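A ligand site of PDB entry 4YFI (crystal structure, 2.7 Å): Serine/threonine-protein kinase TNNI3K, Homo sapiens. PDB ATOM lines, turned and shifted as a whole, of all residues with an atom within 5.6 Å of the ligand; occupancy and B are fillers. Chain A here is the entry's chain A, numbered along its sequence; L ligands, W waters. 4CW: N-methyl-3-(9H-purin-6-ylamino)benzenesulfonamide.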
ATOM      1  N   ILE A  69      21.204 -37.038   8.526  1.00  0.00           N
ATOM      2  CA  ILE A  69      20.189 -36.102   8.055  1.00  0.00           C
ATOM      3  C   ILE A  69      20.435 -35.610   6.638  1.00  0.00           C
ATOM      4  O   ILE A  69      19.574 -34.922   6.092  1.00  0.00           O
ATOM      5  CB  ILE A  69      20.032 -34.895   9.014  1.00  0.00           C
ATOM      6  CG1 ILE A  69      21.332 -34.087   9.081  1.00  0.00           C
ATOM      7  CG2 ILE A  69      19.583 -35.392  10.390  1.00  0.00           C
ATOM      8  CD1 ILE A  69      21.238 -32.827   9.917  1.00  0.00           C
ATOM      9  N   GLY A  70      21.570 -35.967   6.041  1.00  0.00           N
ATOM     10  CA  GLY A  70      21.903 -35.556   4.670  1.00  0.00           C
ATOM     11  C   GLY A  70      22.886 -36.506   4.029  1.00  0.00           C
ATOM     12  O   GLY A  70      23.598 -37.219   4.724  1.00  0.00           O
ATOM     13  N   PHE A  74      30.156 -36.797  -1.774  1.00  0.00           N
ATOM     14  CA  PHE A  74      31.209 -36.287  -0.873  1.00  0.00           C
ATOM     15  C   PHE A  74      31.351 -37.078   0.437  1.00  0.00           C
ATOM     16  O   PHE A  74      32.451 -37.261   0.958  1.00  0.00           O
ATOM     17  CB  PHE A  74      30.980 -34.781  -0.557  1.00  0.00           C
ATOM     18  CG  PHE A  74      29.566 -34.411  -0.144  1.00  0.00           C
ATOM     19  CD1 PHE A  74      29.060 -34.767   1.105  1.00  0.00           C
ATOM     20  CD2 PHE A  74      28.752 -33.655  -0.991  1.00  0.00           C
ATOM     21  CE1 PHE A  74      27.771 -34.414   1.480  1.00  0.00           C
ATOM     22  CE2 PHE A  74      27.455 -33.307  -0.612  1.00  0.00           C
ATOM     23  CZ  PHE A  74      26.971 -33.684   0.625  1.00  0.00           C
ATOM     24  N   VAL A  77      25.971 -36.356   6.106  1.00  0.00           N
ATOM     25  CA  VAL A  77      25.680 -35.305   7.074  1.00  0.00           C
ATOM     26  C   VAL A  77      24.868 -35.841   8.250  1.00  0.00           C
ATOM     27  O   VAL A  77      23.872 -36.534   8.052  1.00  0.00           O
ATOM     28  CB  VAL A  77      24.925 -34.137   6.421  1.00  0.00           C
ATOM     29  CG1 VAL A  77      24.634 -33.053   7.445  1.00  0.00           C
ATOM     30  CG2 VAL A  77      25.738 -33.582   5.267  1.00  0.00           C
ATOM     31  N   ALA A  88      25.380 -29.925  13.408  1.00  0.00           N
ATOM     32  CA  ALA A  88      25.319 -30.679  12.176  1.00  0.00           C
ATOM     33  C   ALA A  88      26.756 -30.926  11.695  1.00  0.00           C
ATOM     34  O   ALA A  88      27.553 -29.989  11.657  1.00  0.00           O
ATOM     35  CB  ALA A  88      24.507 -29.930  11.130  1.00  0.00           C
ATOM     36  N   ILE A  89      27.071 -32.164  11.332  1.00  0.00           N
ATOM     37  CA  ILE A  89      28.419 -32.518  10.898  1.00  0.00           C
ATOM     38  C   ILE A  89      28.431 -33.141   9.533  1.00  0.00           C
ATOM     39  O   ILE A  89      27.853 -34.210   9.319  1.00  0.00           O
ATOM     40  CB  ILE A  89      29.107 -33.530  11.850  1.00  0.00           C
ATOM     41  CG1 ILE A  89      28.875 -33.167  13.319  1.00  0.00           C
ATOM     42  CG2 ILE A  89      30.589 -33.596  11.528  1.00  0.00           C
ATOM     43  CD1 ILE A  89      27.665 -33.836  13.948  1.00  0.00           C
ATOM     44  N   LYS A  90      29.136 -32.503   8.601  1.00  0.00           N
ATOM     45  CA  LYS A  90      29.470 -33.142   7.335  1.00  0.00           C
ATOM     46  C   LYS A  90      30.749 -33.969   7.477  1.00  0.00           C
ATOM     47  O   LYS A  90      31.822 -33.421   7.767  1.00  0.00           O
ATOM     48  CB  LYS A  90      29.650 -32.104   6.236  1.00  0.00           C
ATOM     49  CG  LYS A  90      30.260 -32.677   4.975  1.00  0.00           C
ATOM     50  CD  LYS A  90      30.391 -31.643   3.882  1.00  0.00           C
ATOM     51  CE  LYS A  90      29.041 -31.313   3.303  1.00  0.00           C
ATOM     52  NZ  LYS A  90      29.259 -30.425   2.144  1.00  0.00           N
ATOM     53  N   GLU A 109      36.213 -25.684   0.946  1.00  0.00           N
ATOM     54  CA  GLU A 109      34.923 -25.596   1.631  1.00  0.00           C
ATOM     55  C   GLU A 109      35.079 -24.953   3.000  1.00  0.00           C
ATOM     56  O   GLU A 109      34.242 -24.119   3.398  1.00  0.00           O
ATOM     57  CB  GLU A 109      34.226 -26.954   1.753  1.00  0.00           C
ATOM     58  CG  GLU A 109      32.899 -26.859   2.517  1.00  0.00           C
ATOM     59  CD  GLU A 109      31.961 -28.041   2.306  1.00  0.00           C
ATOM     60  OE1 GLU A 109      32.454 -29.120   1.919  1.00  0.00           O
ATOM     61  OE2 GLU A 109      30.736 -27.882   2.526  1.00  0.00           O
ATOM     62  N   LEU A 113      33.578 -21.341   4.334  1.00  0.00           N
ATOM     63  CA  LEU A 113      32.780 -21.359   5.560  1.00  0.00           C
ATOM     64  C   LEU A 113      33.220 -20.349   6.631  1.00  0.00           C
ATOM     65  O   LEU A 113      32.382 -19.653   7.202  1.00  0.00           O
ATOM     66  CB  LEU A 113      32.716 -22.767   6.159  1.00  0.00           C
ATOM     67  CG  LEU A 113      31.800 -23.747   5.431  1.00  0.00           C
ATOM     68  CD1 LEU A 113      32.059 -25.168   5.896  1.00  0.00           C
ATOM     69  CD2 LEU A 113      30.320 -23.396   5.593  1.00  0.00           C
ATOM     70  N   ILE A 122      24.533 -20.185   6.740  1.00  0.00           N
ATOM     71  CA  ILE A 122      24.918 -21.161   7.777  1.00  0.00           C
ATOM     72  C   ILE A 122      26.092 -20.708   8.655  1.00  0.00           C
ATOM     73  O   ILE A 122      27.023 -20.066   8.184  1.00  0.00           O
ATOM     74  CB  ILE A 122      25.222 -22.547   7.151  1.00  0.00           C
ATOM     75  CG1 ILE A 122      25.024 -23.669   8.173  1.00  0.00           C
ATOM     76  CG2 ILE A 122      26.627 -22.615   6.537  1.00  0.00           C
ATOM     77  CD1 ILE A 122      23.575 -23.973   8.465  1.00  0.00           C
ATOM     78  N   ILE A 137      33.263 -31.333   8.948  1.00  0.00           N
ATOM     79  CA  ILE A 137      32.863 -29.936   8.966  1.00  0.00           C
ATOM     80  C   ILE A 137      31.649 -29.757   9.868  1.00  0.00           C
ATOM     81  O   ILE A 137      30.614 -30.365   9.617  1.00  0.00           O
ATOM     82  CB  ILE A 137      32.538 -29.445   7.540  1.00  0.00           C
ATOM     83  CG1 ILE A 137      33.832 -29.391   6.716  1.00  0.00           C
ATOM     84  CG2 ILE A 137      31.818 -28.103   7.602  1.00  0.00           C
ATOM     85  CD1 ILE A 137      33.698 -28.847   5.300  1.00  0.00           C
ATOM     86  N   VAL A 138      31.775 -28.915  10.891  1.00  0.00           N
ATOM     87  CA  VAL A 138      30.679 -28.708  11.837  1.00  0.00           C
ATOM     88  C   VAL A 138      30.039 -27.320  11.707  1.00  0.00           C
ATOM     89  O   VAL A 138      30.731 -26.303  11.680  1.00  0.00           O
ATOM     90  CB  VAL A 138      31.146 -28.916  13.276  1.00  0.00           C
ATOM     91  CG1 VAL A 138      29.957 -29.117  14.211  1.00  0.00           C
ATOM     92  CG2 VAL A 138      32.060 -30.118  13.346  1.00  0.00           C
ATOM     93  N   THR A 139      28.723 -27.294  11.664  1.00  0.00           N
ATOM     94  CA  THR A 139      27.954 -26.047  11.633  1.00  0.00           C
ATOM     95  C   THR A 139      26.808 -26.135  12.628  1.00  0.00           C
ATOM     96  O   THR A 139      26.546 -27.211  13.195  1.00  0.00           O
ATOM     97  CB  THR A 139      27.295 -25.855  10.263  1.00  0.00           C
ATOM     98  OG1 THR A 139      26.286 -26.850  10.081  1.00  0.00           O
ATOM     99  CG2 THR A 139      28.316 -25.959   9.122  1.00  0.00           C
ATOM    100  N   GLN A 140      26.086 -25.034  12.811  1.00  0.00           N
ATOM    101  CA  GLN A 140      24.860 -25.047  13.616  1.00  0.00           C
ATOM    102  C   GLN A 140      23.908 -26.130  13.125  1.00  0.00           C
ATOM    103  O   GLN A 140      23.930 -26.508  11.958  1.00  0.00           O
ATOM    104  CB  GLN A 140      24.139 -23.711  13.561  1.00  0.00           C
ATOM    105  CG  GLN A 140      23.596 -23.319  12.203  1.00  0.00           C
ATOM    106  CD  GLN A 140      22.987 -21.914  12.205  1.00  0.00           C
ATOM    107  OE1 GLN A 140      23.336 -21.064  11.379  1.00  0.00           O
ATOM    108  NE2 GLN A 140      22.064 -21.660  13.149  1.00  0.00           N
ATOM    109  N   TYR A 141      23.096 -26.639  14.054  1.00  0.00           N
ATOM    110  CA  TYR A 141      21.980 -27.506  13.694  1.00  0.00           C
ATOM    111  C   TYR A 141      20.662 -26.692  13.798  1.00  0.00           C
ATOM    112  O   TYR A 141      20.467 -25.875  14.701  1.00  0.00           O
ATOM    113  CB  TYR A 141      21.926 -28.751  14.592  1.00  0.00           C
ATOM    114  CG  TYR A 141      20.684 -29.574  14.386  1.00  0.00           C
ATOM    115  CD1 TYR A 141      20.553 -30.449  13.297  1.00  0.00           C
ATOM    116  CD2 TYR A 141      19.587 -29.426  15.243  1.00  0.00           C
ATOM    117  CE1 TYR A 141      19.393 -31.170  13.093  1.00  0.00           C
ATOM    118  CE2 TYR A 141      18.426 -30.151  15.052  1.00  0.00           C
ATOM    119  CZ  TYR A 141      18.324 -31.015  13.980  1.00  0.00           C
ATOM    120  OH  TYR A 141      17.152 -31.718  13.818  1.00  0.00           O
ATOM    121  N   ILE A 142      19.763 -26.924  12.858  1.00  0.00           N
ATOM    122  CA  ILE A 142      18.563 -26.125  12.764  1.00  0.00           C
ATOM    123  C   ILE A 142      17.404 -27.098  12.822  1.00  0.00           C
ATOM    124  O   ILE A 142      17.231 -27.947  11.955  1.00  0.00           O
ATOM    125  CB  ILE A 142      18.579 -25.247  11.493  1.00  0.00           C
ATOM    126  CG1 ILE A 142      19.787 -24.299  11.548  1.00  0.00           C
ATOM    127  CG2 ILE A 142      17.265 -24.476  11.364  1.00  0.00           C
ATOM    128  CD1 ILE A 142      19.888 -23.336  10.396  1.00  0.00           C
ATOM    129  N   SER A 143      16.618 -26.974  13.879  1.00  0.00           N
ATOM    130  CA  SER A 143      15.682 -28.012  14.298  1.00  0.00           C
ATOM    131  C   SER A 143      14.392 -28.052  13.474  1.00  0.00           C
ATOM    132  O   SER A 143      13.656 -29.047  13.502  1.00  0.00           O
ATOM    133  CB  SER A 143      15.346 -27.802  15.781  1.00  0.00           C
ATOM    134  OG  SER A 143      14.392 -26.762  15.944  1.00  0.00           O
ATOM    135  N   GLY A 145      14.219 -28.085  10.218  1.00  0.00           N
ATOM    136  CA  GLY A 145      14.404 -28.929   9.031  1.00  0.00           C
ATOM    137  C   GLY A 145      14.525 -28.172   7.729  1.00  0.00           C
ATOM    138  O   GLY A 145      14.555 -26.940   7.699  1.00  0.00           O
ATOM    139  N   SER A 146      14.612 -28.916   6.629  1.00  0.00           N
ATOM    140  CA  SER A 146      14.877 -28.308   5.345  1.00  0.00           C
ATOM    141  C   SER A 146      13.546 -27.864   4.769  1.00  0.00           C
ATOM    142  O   SER A 146      12.474 -28.394   5.143  1.00  0.00           O
ATOM    143  CB  SER A 146      15.544 -29.290   4.393  1.00  0.00           C
ATOM    144  OG  SER A 146      14.600 -30.247   3.924  1.00  0.00           O
ATOM    145  N   HIS A 192      16.516 -28.499  -0.561  1.00  0.00           N
ATOM    146  CA  HIS A 192      17.237 -29.288   0.450  1.00  0.00           C
ATOM    147  C   HIS A 192      18.215 -28.427   1.231  1.00  0.00           C
ATOM    148  O   HIS A 192      18.495 -28.714   2.402  1.00  0.00           O
ATOM    149  CB  HIS A 192      18.034 -30.464  -0.148  1.00  0.00           C
ATOM    150  CG  HIS A 192      17.213 -31.419  -0.958  1.00  0.00           C
ATOM    151  ND1 HIS A 192      16.348 -32.332  -0.380  1.00  0.00           N
ATOM    152  CD2 HIS A 192      17.141 -31.619  -2.291  1.00  0.00           C
ATOM    153  CE1 HIS A 192      15.763 -33.031  -1.337  1.00  0.00           C
ATOM    154  NE2 HIS A 192      16.224 -32.615  -2.504  1.00  0.00           N
ATOM    155  N   ASN A 193      18.767 -27.395   0.575  1.00  0.00           N
ATOM    156  CA  ASN A 193      19.853 -26.550   1.141  1.00  0.00           C
ATOM    157  C   ASN A 193      19.390 -25.205   1.690  1.00  0.00           C
ATOM    158  O   ASN A 193      20.191 -24.335   1.970  1.00  0.00           O
ATOM    159  CB  ASN A 193      20.924 -26.321   0.076  1.00  0.00           C
ATOM    160  CG  ASN A 193      21.659 -27.607  -0.266  1.00  0.00           C
ATOM    161  OD1 ASN A 193      21.736 -28.510   0.565  1.00  0.00           O
ATOM    162  ND2 ASN A 193      22.190 -27.698  -1.489  1.00  0.00           N
ATOM    163  N   LEU A 195      17.422 -24.068   5.010  1.00  0.00           N
ATOM    164  CA  LEU A 195      17.049 -24.663   6.288  1.00  0.00           C
ATOM    165  C   LEU A 195      16.162 -23.703   7.047  1.00  0.00           C
ATOM    166  O   LEU A 195      16.208 -22.508   6.788  1.00  0.00           O
ATOM    167  CB  LEU A 195      18.293 -25.045   7.075  1.00  0.00           C
ATOM    168  CG  LEU A 195      19.300 -25.883   6.272  1.00  0.00           C
ATOM    169  CD1 LEU A 195      20.606 -26.052   7.042  1.00  0.00           C
ATOM    170  CD2 LEU A 195      18.698 -27.251   5.952  1.00  0.00           C
ATOM    171  N   ALA A 205      22.419 -23.168   3.267  1.00  0.00           N
ATOM    172  CA  ALA A 205      23.383 -24.098   3.837  1.00  0.00           C
ATOM    173  C   ALA A 205      24.044 -24.930   2.739  1.00  0.00           C
ATOM    174  O   ALA A 205      23.700 -24.806   1.570  1.00  0.00           O
ATOM    175  CB  ALA A 205      22.676 -25.010   4.835  1.00  0.00           C
ATOM    176  N   ASP A 206      25.008 -25.741   3.161  1.00  0.00           N
ATOM    177  CA  ASP A 206      25.794 -26.608   2.282  1.00  0.00           C
ATOM    178  C   ASP A 206      26.553 -25.855   1.194  1.00  0.00           C
ATOM    179  O   ASP A 206      26.065 -25.640   0.094  1.00  0.00           O
ATOM    180  CB  ASP A 206      24.960 -27.733   1.654  1.00  0.00           C
ATOM    181  CG  ASP A 206      25.832 -28.866   1.091  1.00  0.00           C
ATOM    182  OD1 ASP A 206      27.093 -28.772   1.135  1.00  0.00           O
ATOM    183  OD2 ASP A 206      25.265 -29.862   0.609  1.00  0.00           O
ATOM    184  N   PHE A 207      27.805 -25.511   1.519  1.00  0.00           N
ATOM    185  CA  PHE A 207      28.673 -24.777   0.600  1.00  0.00           C
ATOM    186  C   PHE A 207      29.651 -25.724  -0.109  1.00  0.00           C
ATOM    187  O   PHE A 207      30.715 -25.312  -0.539  1.00  0.00           O
ATOM    188  CB  PHE A 207      29.363 -23.624   1.359  1.00  0.00           C
ATOM    189  CG  PHE A 207      28.417 -22.469   1.638  1.00  0.00           C
ATOM    190  CD1 PHE A 207      27.450 -22.586   2.622  1.00  0.00           C
ATOM    191  CD2 PHE A 207      28.461 -21.317   0.858  1.00  0.00           C
ATOM    192  CE1 PHE A 207      26.546 -21.559   2.849  1.00  0.00           C
ATOM    193  CE2 PHE A 207      27.577 -20.279   1.085  1.00  0.00           C
ATOM    194  CZ  PHE A 207      26.614 -20.396   2.077  1.00  0.00           C
HETATM  195  N18 4CW L   1      21.738 -30.229   6.877  1.00  0.00           N
HETATM  196  C17 4CW L   1      22.879 -29.986   6.084  1.00  0.00           C
HETATM  197  C13 4CW L   1      23.970 -30.577   3.988  1.00  0.00           C
HETATM  198  C10 4CW L   1      25.045 -29.118   5.547  1.00  0.00           C
HETATM  199  C11 4CW L   1      25.072 -29.779   4.315  1.00  0.00           C
HETATM  200  C20 4CW L   1      21.434 -29.557   8.076  1.00  0.00           C
HETATM  201  C28 4CW L   1      18.082 -30.393   9.099  1.00  0.00           C
HETATM  202  C25 4CW L   1      19.838 -29.132   9.808  1.00  0.00           C
HETATM  203  C32 4CW L   1      23.977 -29.178   6.459  1.00  0.00           C
HETATM  204  C01 4CW L   1      27.226 -29.597   7.916  1.00  0.00           C
HETATM  205  N05 4CW L   1      26.765 -28.223   7.622  1.00  0.00           N
HETATM  206  S07 4CW L   1      26.452 -28.054   5.930  1.00  0.00           S
HETATM  207  O08 4CW L   1      25.966 -26.690   5.756  1.00  0.00           O
HETATM  208  O09 4CW L   1      27.613 -28.421   5.061  1.00  0.00           O
HETATM  209  C15 4CW L   1      22.878 -30.662   4.857  1.00  0.00           C
HETATM  210  N21 4CW L   1      22.323 -28.769   8.682  1.00  0.00           N
HETATM  211  C22 4CW L   1      21.978 -28.129   9.827  1.00  0.00           C
HETATM  212  N24 4CW L   1      20.755 -28.333  10.385  1.00  0.00           N
HETATM  213  N26 4CW L   1      18.504 -29.533  10.131  1.00  0.00           N
HETATM  214  N30 4CW L   1      19.058 -30.557   8.187  1.00  0.00           N
HETATM  215  C31 4CW L   1      20.174 -29.761   8.599  1.00  0.00           C
HETATM  216  O   HOH W   1      28.675 -26.352   4.288  1.00  0.00           O
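The backbone NH (N) of Thr 139 lies within hydrogen-bond range of the backbone carbonyl oxygen (O) of Ala 88, 2.9 Å away. NZ of Lys 90 is in salt-bridge range of OD1 of Asp 206. The backbone NH (N) of Ile 69 lies within hydrogen-bond range of the backbone carbonyl oxygen (O) of Val 77, at 2.8 Å. The backbone carbonyl oxygen (O) of Ile 137 is in hydrogen-bond range of the backbone NH (N) of Lys 90, 2.8 Å away. The side-chain amino group (NZ) of Lys 90 is in salt-bridge range of the side-chain carboxylate (OE2) of Glu 109, 3.0 Å away. The backbone carbonyl oxygen (O) of Gly 70 sits at hydrogen-bond distance from the backbone NH (N) of Val 77 (2.9 Å). The backbone NH (N) of Ala 205 is in hydrogen-bond range of the backbone carbonyl oxygen (O) of Asn 193 (2.8 Å).
Ile 69 touches the ligand. Val 77 touches the ligand. Ala 88 touches the ligand (CB to C22, 3.4 Å). Lys 90 touches the ligand (N to C01, 3.5 Å). Ile 122 touches the ligand. O of Ile 137 touches C01 of the ligand, 3.9 Å away. Gln 140 touches the ligand (O to C22, 3.3 Å). Tyr 141 touches the ligand. Gly 145 touches the ligand. Leu 195 touches the ligand (CD1 to N21, 3.6 Å). Ala 205 touches the ligand. Hydrophobic or aromatic side chains that line the ligand: Ile 69, Val 77, Ala 88, Ile 122, Tyr 141, Ile 142, Leu 195 and Ala 205. 14 residues have an atom within 4 Å of the ligand: Ile 69, Val 77, Ala 88, Lys 90, Ile 122, Ile 137, Thr 139, Gln 140, Tyr 141, Ile 142, Gly 145, Leu 195, Ala 205 and Asp 206. The nearest printed residue that does not touch the ligand is Glu 109 (4.1 Å).
The backbone NH (N) of Ile 142 sits at hydrogen-bond distance from a nitrogen (N24) of the ligand (3.0 Å). O of Ile 142 is in hydrogen-bond range of N26 of the ligand (2.7 Å). OG1 of Thr 139 lies within hydrogen-bond range of N05 of the ligand, at 2.9 Å. N of Asp 206 lies within hydrogen-bond range of O08 of the ligand (2.9 Å).
Water W1 lies within hydrogen-bond range of an oxygen (O09) of the ligand, the backbone NH (N) of Phe 207 and the side-chain carboxylate (OE2) of Glu 109.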
